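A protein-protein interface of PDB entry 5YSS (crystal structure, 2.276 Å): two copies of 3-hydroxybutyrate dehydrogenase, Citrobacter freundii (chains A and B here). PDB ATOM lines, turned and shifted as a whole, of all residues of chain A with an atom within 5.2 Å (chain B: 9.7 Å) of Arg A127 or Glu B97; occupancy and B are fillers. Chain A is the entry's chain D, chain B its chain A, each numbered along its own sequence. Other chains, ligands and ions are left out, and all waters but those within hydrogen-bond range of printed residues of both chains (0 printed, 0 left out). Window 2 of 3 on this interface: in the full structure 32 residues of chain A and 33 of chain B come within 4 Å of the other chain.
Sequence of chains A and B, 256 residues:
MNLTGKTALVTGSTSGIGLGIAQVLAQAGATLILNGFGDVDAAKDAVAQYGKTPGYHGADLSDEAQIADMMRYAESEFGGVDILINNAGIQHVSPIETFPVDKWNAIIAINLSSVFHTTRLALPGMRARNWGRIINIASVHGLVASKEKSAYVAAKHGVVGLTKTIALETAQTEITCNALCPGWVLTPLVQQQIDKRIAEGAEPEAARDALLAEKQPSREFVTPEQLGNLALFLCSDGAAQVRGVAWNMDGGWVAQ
The side-chain carboxylate of Glu A169 sits at hydrogen-bond distance from the backbone NH of Ile B96 (2.9 Å). The guanidinium group (NE) of Arg A127 is in salt-bridge range of the side-chain carboxylate (OE2) of Glu B97 (2.6 Å). N of Glu B148 lies within hydrogen-bond range of OE2 of Glu A169 (2.9 Å).
The backbone NH (N) of Ser B94 sits at hydrogen-bond distance from the backbone carbonyl oxygen (O) of Glu B148. NZ of Lys B147 lies within salt-bridge range of OE2 of Glu B148. The guanidinium group (NH2) of Arg A127 lies within hydrogen-bond range of the backbone carbonyl oxygen (O) of Glu A169, at 2.7 Å.
Among the printed residues, merely in contact across the chains: Leu A123 with Glu B97 (3.3 Å), Glu A169 with Pro B95 (3.6 Å), Arg A120 with Ile B96 (3.7 Å), Leu A123 with Ile B96 (3.8 Å) and Glu A169 with Lys B147 (3.9 Å).
Of the printed residues of chain B, Arg A120 touches Ile B96. Of chain B, only Ile B96 (3.8 Å) and Glu B97 (3.3 Å) come within 4 Å of Leu A123. No residue of chain B comes within 4 Å of Pro A124. No residue of chain B comes within 4 Å of Gly A125. Of chain B, only Glu B97 (2.6 Å) comes within 4 Å of Arg A127. No residue of chain B comes within 4 Å of Ala A128. Of the printed residues of chain B, Glu A169 touches Pro B95 (3.6 Å), Ile B96 (2.9 Å), Lys B147 (3.9 Å) and Glu B148 (2.9 Å). Printed residues of chain A within 4 Å of Pro B95: Glu A169 (3.6 Å). Of the printed residues of chain A, Ile B96 touches Arg A120 (3.7 Å), Leu A123 (3.8 Å) and Glu A169 (2.9 Å). Glu B97 touches two residues of chain A. Printed residues of chain A within 4 Å of Lys B147: Glu A169 (3.9 Å). The nearest residue of chain B that does not touch Arg A127 is Lys B147 (5.8 Å).
Hydrophobic or aromatic side chains of chain B within 4 Å of the printed part of chain A: Ile B96. Along chain B the printed residues that touch a printed residue of chain A span positions 95 to 148. Of the 13 printed residues of chain A, 4 touch a printed residue of chain B. Printed residues of chain A that touch a printed residue of chain B: Arg A120, Leu A123, Arg A127 and Glu A169. Hydrophobic or aromatic side chains of chain A within 4 Å of the printed part of chain B: Leu A123. Among the printed residues, Asp or Glu carboxylates within 4 Å of a Lys or Arg side-chain nitrogen of the other chain: Arg A127 with Glu B97 (2.6 Å).
No position is printed for both chains.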
ATOM      1  N   ARG A 120     -19.715  -4.413  -3.382  1.00  0.00           N
ATOM      2  CA  ARG A 120     -18.415  -5.072  -3.504  1.00  0.00           C
ATOM      3  C   ARG A 120     -17.824  -4.985  -4.917  1.00  0.00           C
ATOM      4  O   ARG A 120     -16.673  -4.591  -5.096  1.00  0.00           O
ATOM      5  CB  ARG A 120     -18.546  -6.550  -3.104  1.00  0.00           C
ATOM      6  CG  ARG A 120     -17.249  -7.258  -2.732  1.00  0.00           C
ATOM      7  CD  ARG A 120     -17.533  -8.637  -2.090  1.00  0.00           C
ATOM      8  NE  ARG A 120     -17.272  -9.748  -3.008  1.00  0.00           N
ATOM      9  CZ  ARG A 120     -18.194 -10.318  -3.781  1.00  0.00           C
ATOM     10  NH1 ARG A 120     -19.443  -9.894  -3.744  1.00  0.00           N
ATOM     11  NH2 ARG A 120     -17.868 -11.317  -4.592  1.00  0.00           N
ATOM     12  N   LEU A 123     -17.729  -1.078  -6.847  1.00  0.00           N
ATOM     13  CA  LEU A 123     -16.930  -0.022  -6.259  1.00  0.00           C
ATOM     14  C   LEU A 123     -15.550   0.163  -6.923  1.00  0.00           C
ATOM     15  O   LEU A 123     -15.130   1.307  -7.097  1.00  0.00           O
ATOM     16  CB  LEU A 123     -16.755  -0.260  -4.762  1.00  0.00           C
ATOM     17  CG  LEU A 123     -17.341   0.825  -3.856  1.00  0.00           C
ATOM     18  CD1 LEU A 123     -16.742   0.738  -2.467  1.00  0.00           C
ATOM     19  CD2 LEU A 123     -17.111   2.201  -4.431  1.00  0.00           C
ATOM     20  N   PRO A 124     -14.837  -0.941  -7.275  1.00  0.00           N
ATOM     21  CA  PRO A 124     -13.519  -0.729  -7.899  1.00  0.00           C
ATOM     22  C   PRO A 124     -13.607   0.169  -9.131  1.00  0.00           C
ATOM     23  O   PRO A 124     -12.920   1.184  -9.177  1.00  0.00           O
ATOM     24  CB  PRO A 124     -13.073  -2.148  -8.276  1.00  0.00           C
ATOM     25  CG  PRO A 124     -13.789  -3.023  -7.306  1.00  0.00           C
ATOM     26  CD  PRO A 124     -15.120  -2.382  -7.107  1.00  0.00           C
ATOM     27  N   GLY A 125     -14.468  -0.188 -10.077  1.00  0.00           N
ATOM     28  CA  GLY A 125     -14.735   0.639 -11.241  1.00  0.00           C
ATOM     29  C   GLY A 125     -15.134   2.062 -10.883  1.00  0.00           C
ATOM     30  O   GLY A 125     -14.697   3.017 -11.526  1.00  0.00           O
ATOM     31  N   MET A 126     -15.951   2.222  -9.845  1.00  0.00           N
ATOM     32  CA  MET A 126     -16.334   3.567  -9.433  1.00  0.00           C
ATOM     33  C   MET A 126     -15.144   4.373  -8.940  1.00  0.00           C
ATOM     34  O   MET A 126     -15.084   5.580  -9.176  1.00  0.00           O
ATOM     35  CB  MET A 126     -17.406   3.516  -8.354  1.00  0.00           C
ATOM     36  CG  MET A 126     -18.797   3.319  -8.896  1.00  0.00           C
ATOM     37  SD  MET A 126     -20.005   3.087  -7.572  1.00  0.00           S
ATOM     38  CE  MET A 126     -21.325   2.287  -8.496  1.00  0.00           C
ATOM     39  N   ARG A 127     -14.208   3.705  -8.261  1.00  0.00           N
ATOM     40  CA  ARG A 127     -13.004   4.364  -7.743  1.00  0.00           C
ATOM     41  C   ARG A 127     -12.039   4.789  -8.855  1.00  0.00           C
ATOM     42  O   ARG A 127     -11.450   5.864  -8.777  1.00  0.00           O
ATOM     43  CB  ARG A 127     -12.265   3.463  -6.732  1.00  0.00           C
ATOM     44  CG  ARG A 127     -12.906   3.430  -5.338  1.00  0.00           C
ATOM     45  CD  ARG A 127     -11.927   2.961  -4.255  1.00  0.00           C
ATOM     46  NE  ARG A 127     -12.581   2.723  -2.965  1.00  0.00           N
ATOM     47  CZ  ARG A 127     -12.646   3.613  -1.975  1.00  0.00           C
ATOM     48  NH1 ARG A 127     -12.095   4.816  -2.117  1.00  0.00           N
ATOM     49  NH2 ARG A 127     -13.261   3.299  -0.840  1.00  0.00           N
ATOM     50  N   ALA A 128     -11.883   3.940  -9.868  1.00  0.00           N
ATOM     51  CA  ALA A 128     -11.082   4.253 -11.058  1.00  0.00           C
ATOM     52  C   ALA A 128     -11.563   5.522 -11.761  1.00  0.00           C
ATOM     53  O   ALA A 128     -10.761   6.363 -12.159  1.00  0.00           O
ATOM     54  CB  ALA A 128     -11.102   3.075 -12.047  1.00  0.00           C
ATOM     55  N   ARG A 129     -12.875   5.651 -11.917  1.00  0.00           N
ATOM     56  CA  ARG A 129     -13.455   6.809 -12.581  1.00  0.00           C
ATOM     57  C   ARG A 129     -13.626   7.956 -11.596  1.00  0.00           C
ATOM     58  O   ARG A 129     -14.003   9.061 -11.982  1.00  0.00           O
ATOM     59  CB  ARG A 129     -14.798   6.443 -13.216  1.00  0.00           C
ATOM     60  CG  ARG A 129     -14.703   5.235 -14.150  1.00  0.00           C
ATOM     61  CD  ARG A 129     -16.034   4.853 -14.781  1.00  0.00           C
ATOM     62  NE  ARG A 129     -16.921   4.157 -13.855  1.00  0.00           N
ATOM     63  CZ  ARG A 129     -16.969   2.837 -13.710  1.00  0.00           C
ATOM     64  NH1 ARG A 129     -16.163   2.060 -14.425  1.00  0.00           N
ATOM     65  NH2 ARG A 129     -17.815   2.298 -12.850  1.00  0.00           N
ATOM     66  N   ASN A 130     -13.338   7.681 -10.327  1.00  0.00           N
ATOM     67  CA  ASN A 130     -13.653   8.594  -9.230  1.00  0.00           C
ATOM     68  C   ASN A 130     -15.032   9.257  -9.327  1.00  0.00           C
ATOM     69  O   ASN A 130     -15.147  10.476  -9.244  1.00  0.00           O
ATOM     70  CB  ASN A 130     -12.605   9.697  -9.110  1.00  0.00           C
ATOM     71  CG  ASN A 130     -12.675  10.403  -7.764  1.00  0.00           C
ATOM     72  OD1 ASN A 130     -12.930   9.771  -6.730  1.00  0.00           O
ATOM     73  ND2 ASN A 130     -12.483  11.711  -7.771  1.00  0.00           N
ATOM     74  N   GLU A 169     -16.079   4.770   3.983  1.00  0.00           N
ATOM     75  CA  GLU A 169     -14.997   4.175   3.216  1.00  0.00           C
ATOM     76  C   GLU A 169     -14.759   4.943   1.907  1.00  0.00           C
ATOM     77  O   GLU A 169     -13.664   4.873   1.334  1.00  0.00           O
ATOM     78  CB  GLU A 169     -15.303   2.697   2.922  1.00  0.00           C
ATOM     79  CG  GLU A 169     -14.786   1.734   3.999  1.00  0.00           C
ATOM     80  CD  GLU A 169     -15.260   0.294   3.799  1.00  0.00           C
ATOM     81  OE1 GLU A 169     -15.211  -0.211   2.655  1.00  0.00           O
ATOM     82  OE2 GLU A 169     -15.690  -0.337   4.791  1.00  0.00           O
ATOM     83  N   THR A 170     -15.787   5.667   1.455  1.00  0.00           N
ATOM     84  CA  THR A 170     -15.714   6.460   0.238  1.00  0.00           C
ATOM     85  C   THR A 170     -15.762   7.957   0.533  1.00  0.00           C
ATOM     86  O   THR A 170     -15.834   8.765  -0.388  1.00  0.00           O
ATOM     87  CB  THR A 170     -16.880   6.133  -0.738  1.00  0.00           C
ATOM     88  OG1 THR A 170     -18.138   6.338  -0.073  1.00  0.00           O
ATOM     89  CG2 THR A 170     -16.789   4.695  -1.265  1.00  0.00           C
ATOM     90  N   THR A 173     -13.820  10.617  -1.548  1.00  0.00           N
ATOM     91  CA  THR A 173     -13.872  10.509  -2.993  1.00  0.00           C
ATOM     92  C   THR A 173     -15.147  11.172  -3.506  1.00  0.00           C
ATOM     93  O   THR A 173     -15.942  11.688  -2.720  1.00  0.00           O
ATOM     94  CB  THR A 173     -13.844   9.052  -3.447  1.00  0.00           C
ATOM     95  OG1 THR A 173     -15.133   8.467  -3.206  1.00  0.00           O
ATOM     96  CG2 THR A 173     -12.770   8.274  -2.698  1.00  0.00           C
ATOM     97  N   ILE A 175     -17.523   9.558  -4.725  1.00  0.00           N
ATOM     98  CA  ILE A 175     -18.512   8.490  -4.650  1.00  0.00           C
ATOM     99  C   ILE A 175     -19.307   8.635  -3.358  1.00  0.00           C
ATOM    100  O   ILE A 175     -18.716   8.694  -2.271  1.00  0.00           O
ATOM    101  CB  ILE A 175     -17.844   7.101  -4.667  1.00  0.00           C
ATOM    102  CG1 ILE A 175     -16.922   6.951  -5.885  1.00  0.00           C
ATOM    103  CG2 ILE A 175     -18.883   5.976  -4.548  1.00  0.00           C
ATOM    104  CD1 ILE A 175     -15.970   5.774  -5.774  1.00  0.00           C
ATOM    105  N   HIS B  92     -14.011  -8.956  11.452  1.00  0.00           N
ATOM    106  CA  HIS B  92     -13.019  -8.953  10.384  1.00  0.00           C
ATOM    107  C   HIS B  92     -12.922  -7.543   9.855  1.00  0.00           C
ATOM    108  O   HIS B  92     -13.907  -7.009   9.338  1.00  0.00           O
ATOM    109  CB  HIS B  92     -13.383  -9.922   9.262  1.00  0.00           C
ATOM    110  CG  HIS B  92     -12.382  -9.947   8.159  1.00  0.00           C
ATOM    111  ND1 HIS B  92     -11.098 -10.418   8.330  1.00  0.00           N
ATOM    112  CD2 HIS B  92     -12.462  -9.535   6.865  1.00  0.00           C
ATOM    113  CE1 HIS B  92     -10.434 -10.303   7.194  1.00  0.00           C
ATOM    114  NE2 HIS B  92     -11.238  -9.769   6.291  1.00  0.00           N
ATOM    115  N   VAL B  93     -11.750  -6.923   9.993  1.00  0.00           N
ATOM    116  CA  VAL B  93     -11.605  -5.549   9.524  1.00  0.00           C
ATOM    117  C   VAL B  93     -11.071  -5.497   8.103  1.00  0.00           C
ATOM    118  O   VAL B  93      -9.941  -5.912   7.837  1.00  0.00           O
ATOM    119  CB  VAL B  93     -10.690  -4.713  10.433  1.00  0.00           C
ATOM    120  CG1 VAL B  93     -10.656  -3.286   9.921  1.00  0.00           C
ATOM    121  CG2 VAL B  93     -11.202  -4.733  11.861  1.00  0.00           C
ATOM    122  N   SER B  94     -11.882  -4.977   7.188  1.00  0.00           N
ATOM    123  CA  SER B  94     -11.487  -4.913   5.789  1.00  0.00           C
ATOM    124  C   SER B  94     -12.296  -3.894   5.001  1.00  0.00           C
ATOM    125  O   SER B  94     -13.499  -3.747   5.228  1.00  0.00           O
ATOM    126  CB  SER B  94     -11.615  -6.296   5.140  1.00  0.00           C
ATOM    127  OG  SER B  94     -11.336  -6.235   3.749  1.00  0.00           O
ATOM    128  N   PRO B  95     -11.626  -3.164   4.085  1.00  0.00           N
ATOM    129  CA  PRO B  95     -12.350  -2.383   3.072  1.00  0.00           C
ATOM    130  C   PRO B  95     -13.286  -3.323   2.328  1.00  0.00           C
ATOM    131  O   PRO B  95     -12.898  -4.474   2.126  1.00  0.00           O
ATOM    132  CB  PRO B  95     -11.233  -1.831   2.153  1.00  0.00           C
ATOM    133  CG  PRO B  95      -9.973  -2.554   2.553  1.00  0.00           C
ATOM    134  CD  PRO B  95     -10.160  -2.999   3.980  1.00  0.00           C
ATOM    135  N   ILE B  96     -14.483  -2.875   1.947  1.00  0.00           N
ATOM    136  CA  ILE B  96     -15.492  -3.806   1.452  1.00  0.00           C
ATOM    137  C   ILE B  96     -15.053  -4.520   0.160  1.00  0.00           C
ATOM    138  O   ILE B  96     -15.323  -5.716  -0.015  1.00  0.00           O
ATOM    139  CB  ILE B  96     -16.863  -3.098   1.243  1.00  0.00           C
ATOM    140  CG1 ILE B  96     -17.954  -4.127   0.918  1.00  0.00           C
ATOM    141  CG2 ILE B  96     -16.786  -1.982   0.169  1.00  0.00           C
ATOM    142  CD1 ILE B  96     -19.372  -3.622   1.124  1.00  0.00           C
ATOM    143  N   GLU B  97     -14.355  -3.795  -0.716  1.00  0.00           N
ATOM    144  CA  GLU B  97     -13.865  -4.330  -1.987  1.00  0.00           C
ATOM    145  C   GLU B  97     -13.097  -5.637  -1.851  1.00  0.00           C
ATOM    146  O   GLU B  97     -13.284  -6.553  -2.643  1.00  0.00           O
ATOM    147  CB  GLU B  97     -12.975  -3.300  -2.680  1.00  0.00           C
ATOM    148  CG  GLU B  97     -13.699  -2.016  -3.052  1.00  0.00           C
ATOM    149  CD  GLU B  97     -13.413  -0.872  -2.090  1.00  0.00           C
ATOM    150  OE1 GLU B  97     -13.161  -1.123  -0.884  1.00  0.00           O
ATOM    151  OE2 GLU B  97     -13.437   0.291  -2.551  1.00  0.00           O
ATOM    152  N   THR B  98     -12.238  -5.730  -0.841  1.00  0.00           N
ATOM    153  CA  THR B  98     -11.442  -6.933  -0.644  1.00  0.00           C
ATOM    154  C   THR B  98     -11.906  -7.710   0.598  1.00  0.00           C
ATOM    155  O   THR B  98     -11.111  -8.390   1.256  1.00  0.00           O
ATOM    156  CB  THR B  98      -9.935  -6.587  -0.525  1.00  0.00           C
ATOM    157  OG1 THR B  98      -9.751  -5.605   0.499  1.00  0.00           O
ATOM    158  CG2 THR B  98      -9.412  -6.019  -1.832  1.00  0.00           C
ATOM    159  N   PHE B  99     -13.194  -7.608   0.909  1.00  0.00           N
ATOM    160  CA  PHE B  99     -13.770  -8.281   2.071  1.00  0.00           C
ATOM    161  C   PHE B  99     -14.187  -9.707   1.708  1.00  0.00           C
ATOM    162  O   PHE B  99     -15.135  -9.900   0.962  1.00  0.00           O
ATOM    163  CB  PHE B  99     -14.969  -7.491   2.603  1.00  0.00           C
ATOM    164  CG  PHE B  99     -15.301  -7.769   4.046  1.00  0.00           C
ATOM    165  CD1 PHE B  99     -15.876  -8.973   4.427  1.00  0.00           C
ATOM    166  CD2 PHE B  99     -15.056  -6.812   5.019  1.00  0.00           C
ATOM    167  CE1 PHE B  99     -16.187  -9.220   5.748  1.00  0.00           C
ATOM    168  CE2 PHE B  99     -15.368  -7.052   6.344  1.00  0.00           C
ATOM    169  CZ  PHE B  99     -15.938  -8.261   6.708  1.00  0.00           C
ATOM    170  N   PRO B 100     -13.479 -10.713   2.249  1.00  0.00           N
ATOM    171  CA  PRO B 100     -13.770 -12.112   1.912  1.00  0.00           C
ATOM    172  C   PRO B 100     -15.241 -12.490   2.123  1.00  0.00           C
ATOM    173  O   PRO B 100     -15.866 -12.130   3.138  1.00  0.00           O
ATOM    174  CB  PRO B 100     -12.861 -12.898   2.862  1.00  0.00           C
ATOM    175  CG  PRO B 100     -11.743 -11.956   3.166  1.00  0.00           C
ATOM    176  CD  PRO B 100     -12.380 -10.599   3.221  1.00  0.00           C
ATOM    177  N   VAL B 101     -15.781 -13.213   1.152  1.00  0.00           N
ATOM    178  CA  VAL B 101     -17.155 -13.676   1.210  1.00  0.00           C
ATOM    179  C   VAL B 101     -17.388 -14.553   2.445  1.00  0.00           C
ATOM    180  O   VAL B 101     -18.340 -14.333   3.201  1.00  0.00           O
ATOM    181  CB  VAL B 101     -17.518 -14.444  -0.074  1.00  0.00           C
ATOM    182  CG1 VAL B 101     -18.979 -14.832  -0.074  1.00  0.00           C
ATOM    183  CG2 VAL B 101     -17.209 -13.584  -1.285  1.00  0.00           C
ATOM    184  N   LYS B 147     -15.314   2.708   9.783  1.00  0.00           N
ATOM    185  CA  LYS B 147     -14.689   2.316   8.523  1.00  0.00           C
ATOM    186  C   LYS B 147     -14.217   0.859   8.521  1.00  0.00           C
ATOM    187  O   LYS B 147     -13.633   0.410   9.489  1.00  0.00           O
ATOM    188  CB  LYS B 147     -13.510   3.252   8.245  1.00  0.00           C
ATOM    189  CG  LYS B 147     -12.585   2.817   7.140  1.00  0.00           C
ATOM    190  CD  LYS B 147     -11.457   3.834   6.938  1.00  0.00           C
ATOM    191  CE  LYS B 147     -10.486   3.397   5.842  1.00  0.00           C
ATOM    192  NZ  LYS B 147     -11.124   3.023   4.531  1.00  0.00           N
ATOM    193  N   GLU B 148     -14.500   0.132   7.443  1.00  0.00           N
ATOM    194  CA  GLU B 148     -13.949  -1.210   7.194  1.00  0.00           C
ATOM    195  C   GLU B 148     -14.481  -2.327   8.100  1.00  0.00           C
ATOM    196  O   GLU B 148     -13.878  -3.391   8.201  1.00  0.00           O
ATOM    197  CB  GLU B 148     -12.412  -1.160   7.261  1.00  0.00           C
ATOM    198  CG  GLU B 148     -11.826  -0.416   6.049  1.00  0.00           C
ATOM    199  CD  GLU B 148     -10.320  -0.174   6.117  1.00  0.00           C
ATOM    200  OE1 GLU B 148      -9.653  -0.649   7.063  1.00  0.00           O
ATOM    201  OE2 GLU B 148      -9.806   0.498   5.194  1.00  0.00           O
ATOM    202  N   LYS B 149     -15.638  -2.109   8.716  1.00  0.00           N
ATOM    203  CA  LYS B 149     -16.288  -3.164   9.479  1.00  0.00           C
ATOM    204  C   LYS B 149     -17.691  -3.412   8.932  1.00  0.00           C
ATOM    205  O   LYS B 149     -18.667  -3.512   9.688  1.00  0.00           O
ATOM    206  CB  LYS B 149     -16.323  -2.793  10.960  1.00  0.00           C
ATOM    207  CG  LYS B 149     -14.945  -2.676  11.566  1.00  0.00           C
ATOM    208  CD  LYS B 149     -14.976  -2.213  13.012  1.00  0.00           C
ATOM    209  CE  LYS B 149     -13.538  -2.071  13.540  1.00  0.00           C
ATOM    210  NZ  LYS B 149     -13.499  -1.764  14.982  1.00  0.00           N
ATOM    211  N   SER B 150     -17.788  -3.516   7.611  1.00  0.00           N
ATOM    212  CA  SER B 150     -19.091  -3.540   6.957  1.00  0.00           C
ATOM    213  C   SER B 150     -19.953  -4.701   7.456  1.00  0.00           C
ATOM    214  O   SER B 150     -21.118  -4.504   7.815  1.00  0.00           O
ATOM    215  CB  SER B 150     -18.944  -3.594   5.428  1.00  0.00           C
ATOM    216  OG  SER B 150     -18.174  -4.709   5.019  1.00  0.00           O
